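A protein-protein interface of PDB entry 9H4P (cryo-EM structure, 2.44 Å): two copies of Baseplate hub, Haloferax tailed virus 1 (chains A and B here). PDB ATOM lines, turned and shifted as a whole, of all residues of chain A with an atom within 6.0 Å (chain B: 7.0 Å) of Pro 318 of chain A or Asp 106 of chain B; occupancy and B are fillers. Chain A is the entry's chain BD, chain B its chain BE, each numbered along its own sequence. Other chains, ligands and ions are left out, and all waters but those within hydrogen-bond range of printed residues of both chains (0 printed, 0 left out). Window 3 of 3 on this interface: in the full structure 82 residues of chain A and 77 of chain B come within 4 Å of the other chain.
The backbone carbonyl oxygen of Pro 318 of chain A sits at hydrogen-bond distance from the backbone NH of Gly 62 of chain B (3.0 Å).
The side-chain carboxylate of Asp 106 of chain B is in hydrogen-bond range of the side-chain hydroxyl of Tyr 217 of chain A (2.5 Å).
The side-chain carboxylate of Glu 99 of chain B lies within salt-bridge range of the guanidinium group of Arg 319 of chain A (3.4 Å).
The backbone carbonyl oxygen (O) of Tyr 217 of chain A is in hydrogen-bond range of the backbone NH (N) of Glu 101 of chain B (3.1 Å).
N of Asp 317 of chain A lies within hydrogen-bond range of OD1 of Asn 211 of chain A (2.9 Å).
The backbone carbonyl oxygen of Asn 100 of chain B is in hydrogen-bond range of the backbone NH of Val 107 of chain B, 2.9 Å away.
The backbone carbonyl oxygen (O) of Asp 106 of chain B sits at hydrogen-bond distance from the backbone NH (N) of Asp 60 of chain B (3.0 Å).
The side-chain carboxylate of Glu 101 of chain B lies within hydrogen-bond range of the backbone NH of Gly 104 of chain B, at 2.8 Å.
Glu 99 of chain B touches Tyr 217 of chain A (O to CE1, 3.6 Å).
Asn 100 of chain B touches Tyr 217 of chain A.
Asp 317 of chain A touches Gly 62 of chain B (O to CA, 3.9 Å).
O of Pro 318 of chain A touches N of Gly 63 of chain B, at 3.7 Å.
Asp 106 of chain B touches Pro 318 of chain A.
Arg 319 of chain A touches Gly 62 of chain B (C to C, 3.7 Å).
Arg 319 of chain A touches Gly 63 of chain B.
Gly 320 of chain A touches Gly 62 of chain B.
Of chain B, only Gly 62, Gly 63 and Asp 106 come within 4 Å of Pro 318 of chain A.
Asp 106 of chain B touches two residues of chain A.
Of the printed residues of chain B, Gly 320 of chain A touches Gly 62.
Of the printed residues of chain A, Glu 99 of chain B touches Tyr 217 and Arg 319.
Printed residues of chain B within 4 Å of Asp 317 of chain A: Gly 62 (3.9 Å).
Printed residues of chain A within 4 Å of Asn 100 of chain B: Tyr 217 (3.7 Å).
The nearest residue of chain B that does not touch Pro 318 of chain A is Arg 61 of chain B (4.1 Å).
The nearest residue of chain A that does not touch Asp 106 of chain B is Arg 319 of chain A (5.2 Å).
Of the 8 printed residues of chain A, 5 touch a printed residue of chain B.
Of the 18 printed residues of chain B, 6 touch a printed residue of chain A.
Among the printed residues, 12 pairs touch across the chains.
No position is printed for both chains.
Of the 12 pairs that touch across the chains among the printed residues, none has its exchanged pair printed and touching as well.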
ATOM      1  N   ASN A 211      28.875  16.095   0.660  1.00  0.00           N
ATOM      2  CA  ASN A 211      27.537  15.556   0.459  1.00  0.00           C
ATOM      3  C   ASN A 211      27.487  14.022   0.461  1.00  0.00           C
ATOM      4  O   ASN A 211      26.440  13.447   0.717  1.00  0.00           O
ATOM      5  CB  ASN A 211      26.955  16.133  -0.829  1.00  0.00           C
ATOM      6  CG  ASN A 211      25.480  15.822  -0.933  1.00  0.00           C
ATOM      7  OD1 ASN A 211      24.714  16.081  -0.021  1.00  0.00           O
ATOM      8  ND2 ASN A 211      25.037  15.228  -2.008  1.00  0.00           N
ATOM      9  N   TRP A 214      27.758  12.859   5.087  1.00  0.00           N
ATOM     10  CA  TRP A 214      26.666  12.848   6.056  1.00  0.00           C
ATOM     11  C   TRP A 214      25.772  11.639   5.782  1.00  0.00           C
ATOM     12  O   TRP A 214      25.700  11.169   4.652  1.00  0.00           O
ATOM     13  CB  TRP A 214      25.872  14.155   5.963  1.00  0.00           C
ATOM     14  CG  TRP A 214      25.101  14.324   4.700  1.00  0.00           C
ATOM     15  CD1 TRP A 214      25.547  14.934   3.586  1.00  0.00           C
ATOM     16  CD2 TRP A 214      23.780  13.811   4.366  1.00  0.00           C
ATOM     17  NE1 TRP A 214      24.619  14.792   2.582  1.00  0.00           N
ATOM     18  CE2 TRP A 214      23.545  14.047   2.987  1.00  0.00           C
ATOM     19  CE3 TRP A 214      22.767  13.140   5.080  1.00  0.00           C
ATOM     20  CZ2 TRP A 214      22.417  13.564   2.326  1.00  0.00           C
ATOM     21  CZ3 TRP A 214      21.611  12.676   4.434  1.00  0.00           C
ATOM     22  CH2 TRP A 214      21.447  12.867   3.055  1.00  0.00           C
ATOM     23  N   TYR A 217      20.703  13.936   9.404  1.00  0.00           N
ATOM     24  CA  TYR A 217      20.781  15.303   9.907  1.00  0.00           C
ATOM     25  C   TYR A 217      19.459  15.709  10.563  1.00  0.00           C
ATOM     26  O   TYR A 217      18.408  15.143  10.274  1.00  0.00           O
ATOM     27  CB  TYR A 217      21.202  16.256   8.781  1.00  0.00           C
ATOM     28  CG  TYR A 217      20.106  16.515   7.782  1.00  0.00           C
ATOM     29  CD1 TYR A 217      19.113  17.456   8.094  1.00  0.00           C
ATOM     30  CD2 TYR A 217      20.012  15.755   6.603  1.00  0.00           C
ATOM     31  CE1 TYR A 217      17.993  17.589   7.275  1.00  0.00           C
ATOM     32  CE2 TYR A 217      18.903  15.916   5.752  1.00  0.00           C
ATOM     33  CZ  TYR A 217      17.886  16.823   6.106  1.00  0.00           C
ATOM     34  OH  TYR A 217      16.789  16.991   5.342  1.00  0.00           O
ATOM     35  N   ILE A 316      25.207  19.607   2.551  1.00  0.00           N
ATOM     36  CA  ILE A 316      24.076  18.676   2.552  1.00  0.00           C
ATOM     37  C   ILE A 316      23.108  19.131   1.469  1.00  0.00           C
ATOM     38  O   ILE A 316      22.208  19.927   1.724  1.00  0.00           O
ATOM     39  CB  ILE A 316      23.406  18.573   3.942  1.00  0.00           C
ATOM     40  CG1 ILE A 316      24.428  18.272   5.051  1.00  0.00           C
ATOM     41  CG2 ILE A 316      22.300  17.512   3.918  1.00  0.00           C
ATOM     42  CD1 ILE A 316      23.837  18.152   6.452  1.00  0.00           C
ATOM     43  N   ASP A 317      23.293  18.645   0.246  1.00  0.00           N
ATOM     44  CA  ASP A 317      22.529  19.089  -0.921  1.00  0.00           C
ATOM     45  C   ASP A 317      21.020  18.876  -0.783  1.00  0.00           C
ATOM     46  O   ASP A 317      20.278  19.797  -1.118  1.00  0.00           O
ATOM     47  CB  ASP A 317      23.041  18.445  -2.217  1.00  0.00           C
ATOM     48  CG  ASP A 317      24.435  18.904  -2.646  1.00  0.00           C
ATOM     49  OD1 ASP A 317      24.957  19.886  -2.088  1.00  0.00           O
ATOM     50  OD2 ASP A 317      24.986  18.302  -3.592  1.00  0.00           O
ATOM     51  N   PRO A 318      20.514  17.752  -0.234  1.00  0.00           N
ATOM     52  CA  PRO A 318      19.091  17.600   0.035  1.00  0.00           C
ATOM     53  C   PRO A 318      18.494  18.690   0.912  1.00  0.00           C
ATOM     54  O   PRO A 318      17.297  18.945   0.815  1.00  0.00           O
ATOM     55  CB  PRO A 318      18.949  16.248   0.722  1.00  0.00           C
ATOM     56  CG  PRO A 318      20.096  15.455   0.128  1.00  0.00           C
ATOM     57  CD  PRO A 318      21.199  16.501   0.054  1.00  0.00           C
ATOM     58  N   ARG A 319      19.306  19.353   1.742  1.00  0.00           N
ATOM     59  CA  ARG A 319      18.866  20.331   2.735  1.00  0.00           C
ATOM     60  C   ARG A 319      19.384  21.751   2.497  1.00  0.00           C
ATOM     61  O   ARG A 319      19.175  22.627   3.329  1.00  0.00           O
ATOM     62  CB  ARG A 319      19.217  19.797   4.123  1.00  0.00           C
ATOM     63  CG  ARG A 319      18.254  20.378   5.162  1.00  0.00           C
ATOM     64  CD  ARG A 319      19.005  20.873   6.382  1.00  0.00           C
ATOM     65  NE  ARG A 319      18.124  21.635   7.272  1.00  0.00           N
ATOM     66  CZ  ARG A 319      17.852  22.921   7.180  1.00  0.00           C
ATOM     67  NH1 ARG A 319      17.274  23.514   8.179  1.00  0.00           N
ATOM     68  NH2 ARG A 319      18.186  23.646   6.152  1.00  0.00           N
ATOM     69  N   GLY A 320      20.056  21.987   1.377  1.00  0.00           N
ATOM     70  CA  GLY A 320      20.500  23.319   0.966  1.00  0.00           C
ATOM     71  C   GLY A 320      21.616  23.927   1.812  1.00  0.00           C
ATOM     72  O   GLY A 320      21.826  25.134   1.759  1.00  0.00           O
ATOM     73  N   TRP B  39       1.389  17.722   4.697  1.00  0.00           N
ATOM     74  CA  TRP B  39       0.826  16.378   4.783  1.00  0.00           C
ATOM     75  C   TRP B  39       0.308  16.019   6.172  1.00  0.00           C
ATOM     76  O   TRP B  39      -0.324  14.975   6.333  1.00  0.00           O
ATOM     77  CB  TRP B  39       1.848  15.371   4.251  1.00  0.00           C
ATOM     78  CG  TRP B  39       3.176  15.310   4.933  1.00  0.00           C
ATOM     79  CD1 TRP B  39       4.308  15.885   4.483  1.00  0.00           C
ATOM     80  CD2 TRP B  39       3.544  14.642   6.175  1.00  0.00           C
ATOM     81  NE1 TRP B  39       5.342  15.615   5.350  1.00  0.00           N
ATOM     82  CE2 TRP B  39       4.930  14.849   6.406  1.00  0.00           C
ATOM     83  CE3 TRP B  39       2.858  13.862   7.118  1.00  0.00           C
ATOM     84  CZ2 TRP B  39       5.600  14.305   7.503  1.00  0.00           C
ATOM     85  CZ3 TRP B  39       3.508  13.357   8.258  1.00  0.00           C
ATOM     86  CH2 TRP B  39       4.878  13.563   8.445  1.00  0.00           C
ATOM     87  N   MET B  58       5.519  19.151   6.624  1.00  0.00           N
ATOM     88  CA  MET B  58       5.664  19.300   5.182  1.00  0.00           C
ATOM     89  C   MET B  58       6.801  18.442   4.665  1.00  0.00           C
ATOM     90  O   MET B  58       7.721  18.103   5.398  1.00  0.00           O
ATOM     91  CB  MET B  58       5.989  20.748   4.842  1.00  0.00           C
ATOM     92  CG  MET B  58       4.826  21.684   5.094  1.00  0.00           C
ATOM     93  SD  MET B  58       5.353  23.250   5.785  1.00  0.00           S
ATOM     94  CE  MET B  58       5.502  22.806   7.517  1.00  0.00           C
ATOM     95  N   ASP B  59       6.772  18.119   3.382  1.00  0.00           N
ATOM     96  CA  ASP B  59       7.992  17.772   2.660  1.00  0.00           C
ATOM     97  C   ASP B  59       8.727  19.028   2.222  1.00  0.00           C
ATOM     98  O   ASP B  59       8.110  20.035   1.891  1.00  0.00           O
ATOM     99  CB  ASP B  59       7.668  16.941   1.429  1.00  0.00           C
ATOM    100  CG  ASP B  59       7.411  15.497   1.807  1.00  0.00           C
ATOM    101  OD1 ASP B  59       8.392  14.805   2.144  1.00  0.00           O
ATOM    102  OD2 ASP B  59       6.237  15.064   1.769  1.00  0.00           O
ATOM    103  N   ASP B  60      10.044  18.940   2.136  1.00  0.00           N
ATOM    104  CA  ASP B  60      10.878  19.993   1.577  1.00  0.00           C
ATOM    105  C   ASP B  60      11.896  19.450   0.560  1.00  0.00           C
ATOM    106  O   ASP B  60      12.216  18.261   0.531  1.00  0.00           O
ATOM    107  CB  ASP B  60      11.516  20.783   2.726  1.00  0.00           C
ATOM    108  CG  ASP B  60      11.978  22.177   2.299  1.00  0.00           C
ATOM    109  OD1 ASP B  60      11.783  22.530   1.114  1.00  0.00           O
ATOM    110  OD2 ASP B  60      12.460  22.952   3.147  1.00  0.00           O
ATOM    111  N   ARG B  61      12.366  20.321  -0.334  1.00  0.00           N
ATOM    112  CA  ARG B  61      13.362  20.052  -1.368  1.00  0.00           C
ATOM    113  C   ARG B  61      14.475  21.078  -1.217  1.00  0.00           C
ATOM    114  O   ARG B  61      14.196  22.271  -1.270  1.00  0.00           O
ATOM    115  CB  ARG B  61      12.758  20.174  -2.781  1.00  0.00           C
ATOM    116  CG  ARG B  61      11.460  19.423  -3.126  1.00  0.00           C
ATOM    117  CD  ARG B  61      10.135  19.932  -2.528  1.00  0.00           C
ATOM    118  NE  ARG B  61      10.007  21.402  -2.425  1.00  0.00           N
ATOM    119  CZ  ARG B  61      10.054  22.330  -3.367  1.00  0.00           C
ATOM    120  NH1 ARG B  61       9.941  23.583  -3.053  1.00  0.00           N
ATOM    121  NH2 ARG B  61      10.214  22.058  -4.625  1.00  0.00           N
ATOM    122  N   GLY B  62      15.725  20.664  -1.043  1.00  0.00           N
ATOM    123  CA  GLY B  62      16.861  21.591  -0.999  1.00  0.00           C
ATOM    124  C   GLY B  62      16.768  22.668   0.084  1.00  0.00           C
ATOM    125  O   GLY B  62      17.348  23.738  -0.075  1.00  0.00           O
ATOM    126  N   GLY B  63      15.993  22.440   1.143  1.00  0.00           N
ATOM    127  CA  GLY B  63      15.726  23.420   2.198  1.00  0.00           C
ATOM    128  C   GLY B  63      14.912  24.646   1.766  1.00  0.00           C
ATOM    129  O   GLY B  63      14.955  25.670   2.440  1.00  0.00           O
ATOM    130  N   GLN B  64      14.228  24.621   0.623  1.00  0.00           N
ATOM    131  CA  GLN B  64      13.558  25.798   0.075  1.00  0.00           C
ATOM    132  C   GLN B  64      12.339  26.238   0.889  1.00  0.00           C
ATOM    133  O   GLN B  64      12.129  27.436   1.049  1.00  0.00           O
ATOM    134  CB  GLN B  64      13.156  25.525  -1.378  1.00  0.00           C
ATOM    135  CG  GLN B  64      14.378  25.419  -2.297  1.00  0.00           C
ATOM    136  CD  GLN B  64      14.031  25.031  -3.730  1.00  0.00           C
ATOM    137  OE1 GLN B  64      12.882  24.920  -4.133  1.00  0.00           O
ATOM    138  NE2 GLN B  64      15.019  24.837  -4.572  1.00  0.00           N
ATOM    139  N   GLU B  99      14.006  20.810  10.375  1.00  0.00           N
ATOM    140  CA  GLU B  99      14.024  19.931   9.213  1.00  0.00           C
ATOM    141  C   GLU B  99      14.867  18.691   9.475  1.00  0.00           C
ATOM    142  O   GLU B  99      15.954  18.783  10.044  1.00  0.00           O
ATOM    143  CB  GLU B  99      14.456  20.701   7.980  1.00  0.00           C
ATOM    144  CG  GLU B  99      14.213  19.892   6.711  1.00  0.00           C
ATOM    145  CD  GLU B  99      14.714  20.592   5.448  1.00  0.00           C
ATOM    146  OE1 GLU B  99      15.227  21.724   5.556  1.00  0.00           O
ATOM    147  OE2 GLU B  99      14.638  19.980   4.367  1.00  0.00           O
ATOM    148  N   ASN B 100      14.356  17.516   9.132  1.00  0.00           N
ATOM    149  CA  ASN B 100      14.925  16.223   9.498  1.00  0.00           C
ATOM    150  C   ASN B 100      15.051  15.281   8.316  1.00  0.00           C
ATOM    151  O   ASN B 100      14.138  15.150   7.509  1.00  0.00           O
ATOM    152  CB  ASN B 100      14.036  15.539  10.548  1.00  0.00           C
ATOM    153  CG  ASN B 100      14.284  15.977  11.963  1.00  0.00           C
ATOM    154  OD1 ASN B 100      14.020  15.258  12.905  1.00  0.00           O
ATOM    155  ND2 ASN B 100      14.875  17.124  12.158  1.00  0.00           N
ATOM    156  N   GLU B 101      16.123  14.501   8.324  1.00  0.00           N
ATOM    157  CA  GLU B 101      16.171  13.226   7.634  1.00  0.00           C
ATOM    158  C   GLU B 101      15.235  12.245   8.347  1.00  0.00           C
ATOM    159  O   GLU B 101      15.534  11.812   9.457  1.00  0.00           O
ATOM    160  CB  GLU B 101      17.628  12.738   7.663  1.00  0.00           C
ATOM    161  CG  GLU B 101      17.863  11.305   7.175  1.00  0.00           C
ATOM    162  CD  GLU B 101      17.607  11.105   5.690  1.00  0.00           C
ATOM    163  OE1 GLU B 101      17.666  12.078   4.919  1.00  0.00           O
ATOM    164  OE2 GLU B 101      17.392   9.945   5.281  1.00  0.00           O
ATOM    165  N   GLN B 102      14.136  11.842   7.717  1.00  0.00           N
ATOM    166  CA  GLN B 102      13.288  10.751   8.192  1.00  0.00           C
ATOM    167  C   GLN B 102      13.235   9.629   7.157  1.00  0.00           C
ATOM    168  O   GLN B 102      12.404   9.642   6.253  1.00  0.00           O
ATOM    169  CB  GLN B 102      11.887  11.254   8.544  1.00  0.00           C
ATOM    170  CG  GLN B 102      11.855  12.159   9.781  1.00  0.00           C
ATOM    171  CD  GLN B 102      10.453  12.298  10.368  1.00  0.00           C
ATOM    172  OE1 GLN B 102       9.479  11.777   9.849  1.00  0.00           O
ATOM    173  NE2 GLN B 102      10.274  12.988  11.471  1.00  0.00           N
ATOM    174  N   GLN B 103      14.127   8.646   7.265  1.00  0.00           N
ATOM    175  CA  GLN B 103      14.134   7.465   6.392  1.00  0.00           C
ATOM    176  C   GLN B 103      14.132   7.836   4.898  1.00  0.00           C
ATOM    177  O   GLN B 103      13.341   7.305   4.122  1.00  0.00           O
ATOM    178  CB  GLN B 103      12.980   6.522   6.774  1.00  0.00           C
ATOM    179  CG  GLN B 103      12.968   6.079   8.245  1.00  0.00           C
ATOM    180  CD  GLN B 103      11.718   5.281   8.603  1.00  0.00           C
ATOM    181  OE1 GLN B 103      10.941   4.861   7.757  1.00  0.00           O
ATOM    182  NE2 GLN B 103      11.455   5.035   9.865  1.00  0.00           N
ATOM    183  N   GLY B 104      14.929   8.820   4.495  1.00  0.00           N
ATOM    184  CA  GLY B 104      14.976   9.354   3.138  1.00  0.00           C
ATOM    185  C   GLY B 104      14.162  10.626   2.915  1.00  0.00           C
ATOM    186  O   GLY B 104      14.606  11.495   2.174  1.00  0.00           O
ATOM    187  N   ALA B 105      13.024  10.808   3.577  1.00  0.00           N
ATOM    188  CA  ALA B 105      12.256  12.039   3.461  1.00  0.00           C
ATOM    189  C   ALA B 105      12.985  13.203   4.146  1.00  0.00           C
ATOM    190  O   ALA B 105      13.642  13.004   5.160  1.00  0.00           O
ATOM    191  CB  ALA B 105      10.870  11.820   4.064  1.00  0.00           C
ATOM    192  N   ASP B 106      12.847  14.416   3.619  1.00  0.00           N
ATOM    193  CA  ASP B 106      13.302  15.647   4.269  1.00  0.00           C
ATOM    194  C   ASP B 106      12.073  16.349   4.835  1.00  0.00           C
ATOM    195  O   ASP B 106      11.334  17.011   4.111  1.00  0.00           O
ATOM    196  CB  ASP B 106      14.062  16.554   3.300  1.00  0.00           C
ATOM    197  CG  ASP B 106      15.261  15.872   2.650  1.00  0.00           C
ATOM    198  OD1 ASP B 106      16.218  15.502   3.360  1.00  0.00           O
ATOM    199  OD2 ASP B 106      15.228  15.642   1.424  1.00  0.00           O
ATOM    200  N   VAL B 107      11.781  16.114   6.107  1.00  0.00           N
ATOM    201  CA  VAL B 107      10.526  16.549   6.722  1.00  0.00           C
ATOM    202  C   VAL B 107      10.745  17.879   7.399  1.00  0.00           C
ATOM    203  O   VAL B 107      11.602  17.979   8.268  1.00  0.00           O
ATOM    204  CB  VAL B 107      10.023  15.514   7.732  1.00  0.00           C
ATOM    205  CG1 VAL B 107       8.815  16.022   8.513  1.00  0.00           C
ATOM    206  CG2 VAL B 107       9.621  14.233   7.004  1.00  0.00           C
ATOM    207  N   LEU B 108       9.957  18.886   7.042  1.00  0.00           N
ATOM    208  CA  LEU B 108       9.937  20.178   7.702  1.00  0.00           C
ATOM    209  C   LEU B 108       8.785  20.184   8.699  1.00  0.00           C
ATOM    210  O   LEU B 108       7.631  20.055   8.316  1.00  0.00           O
ATOM    211  CB  LEU B 108       9.804  21.262   6.627  1.00  0.00           C
ATOM    212  CG  LEU B 108       9.509  22.674   7.145  1.00  0.00           C
ATOM    213  CD1 LEU B 108      10.644  23.233   7.985  1.00  0.00           C
ATOM    214  CD2 LEU B 108       9.300  23.615   5.974  1.00  0.00           C
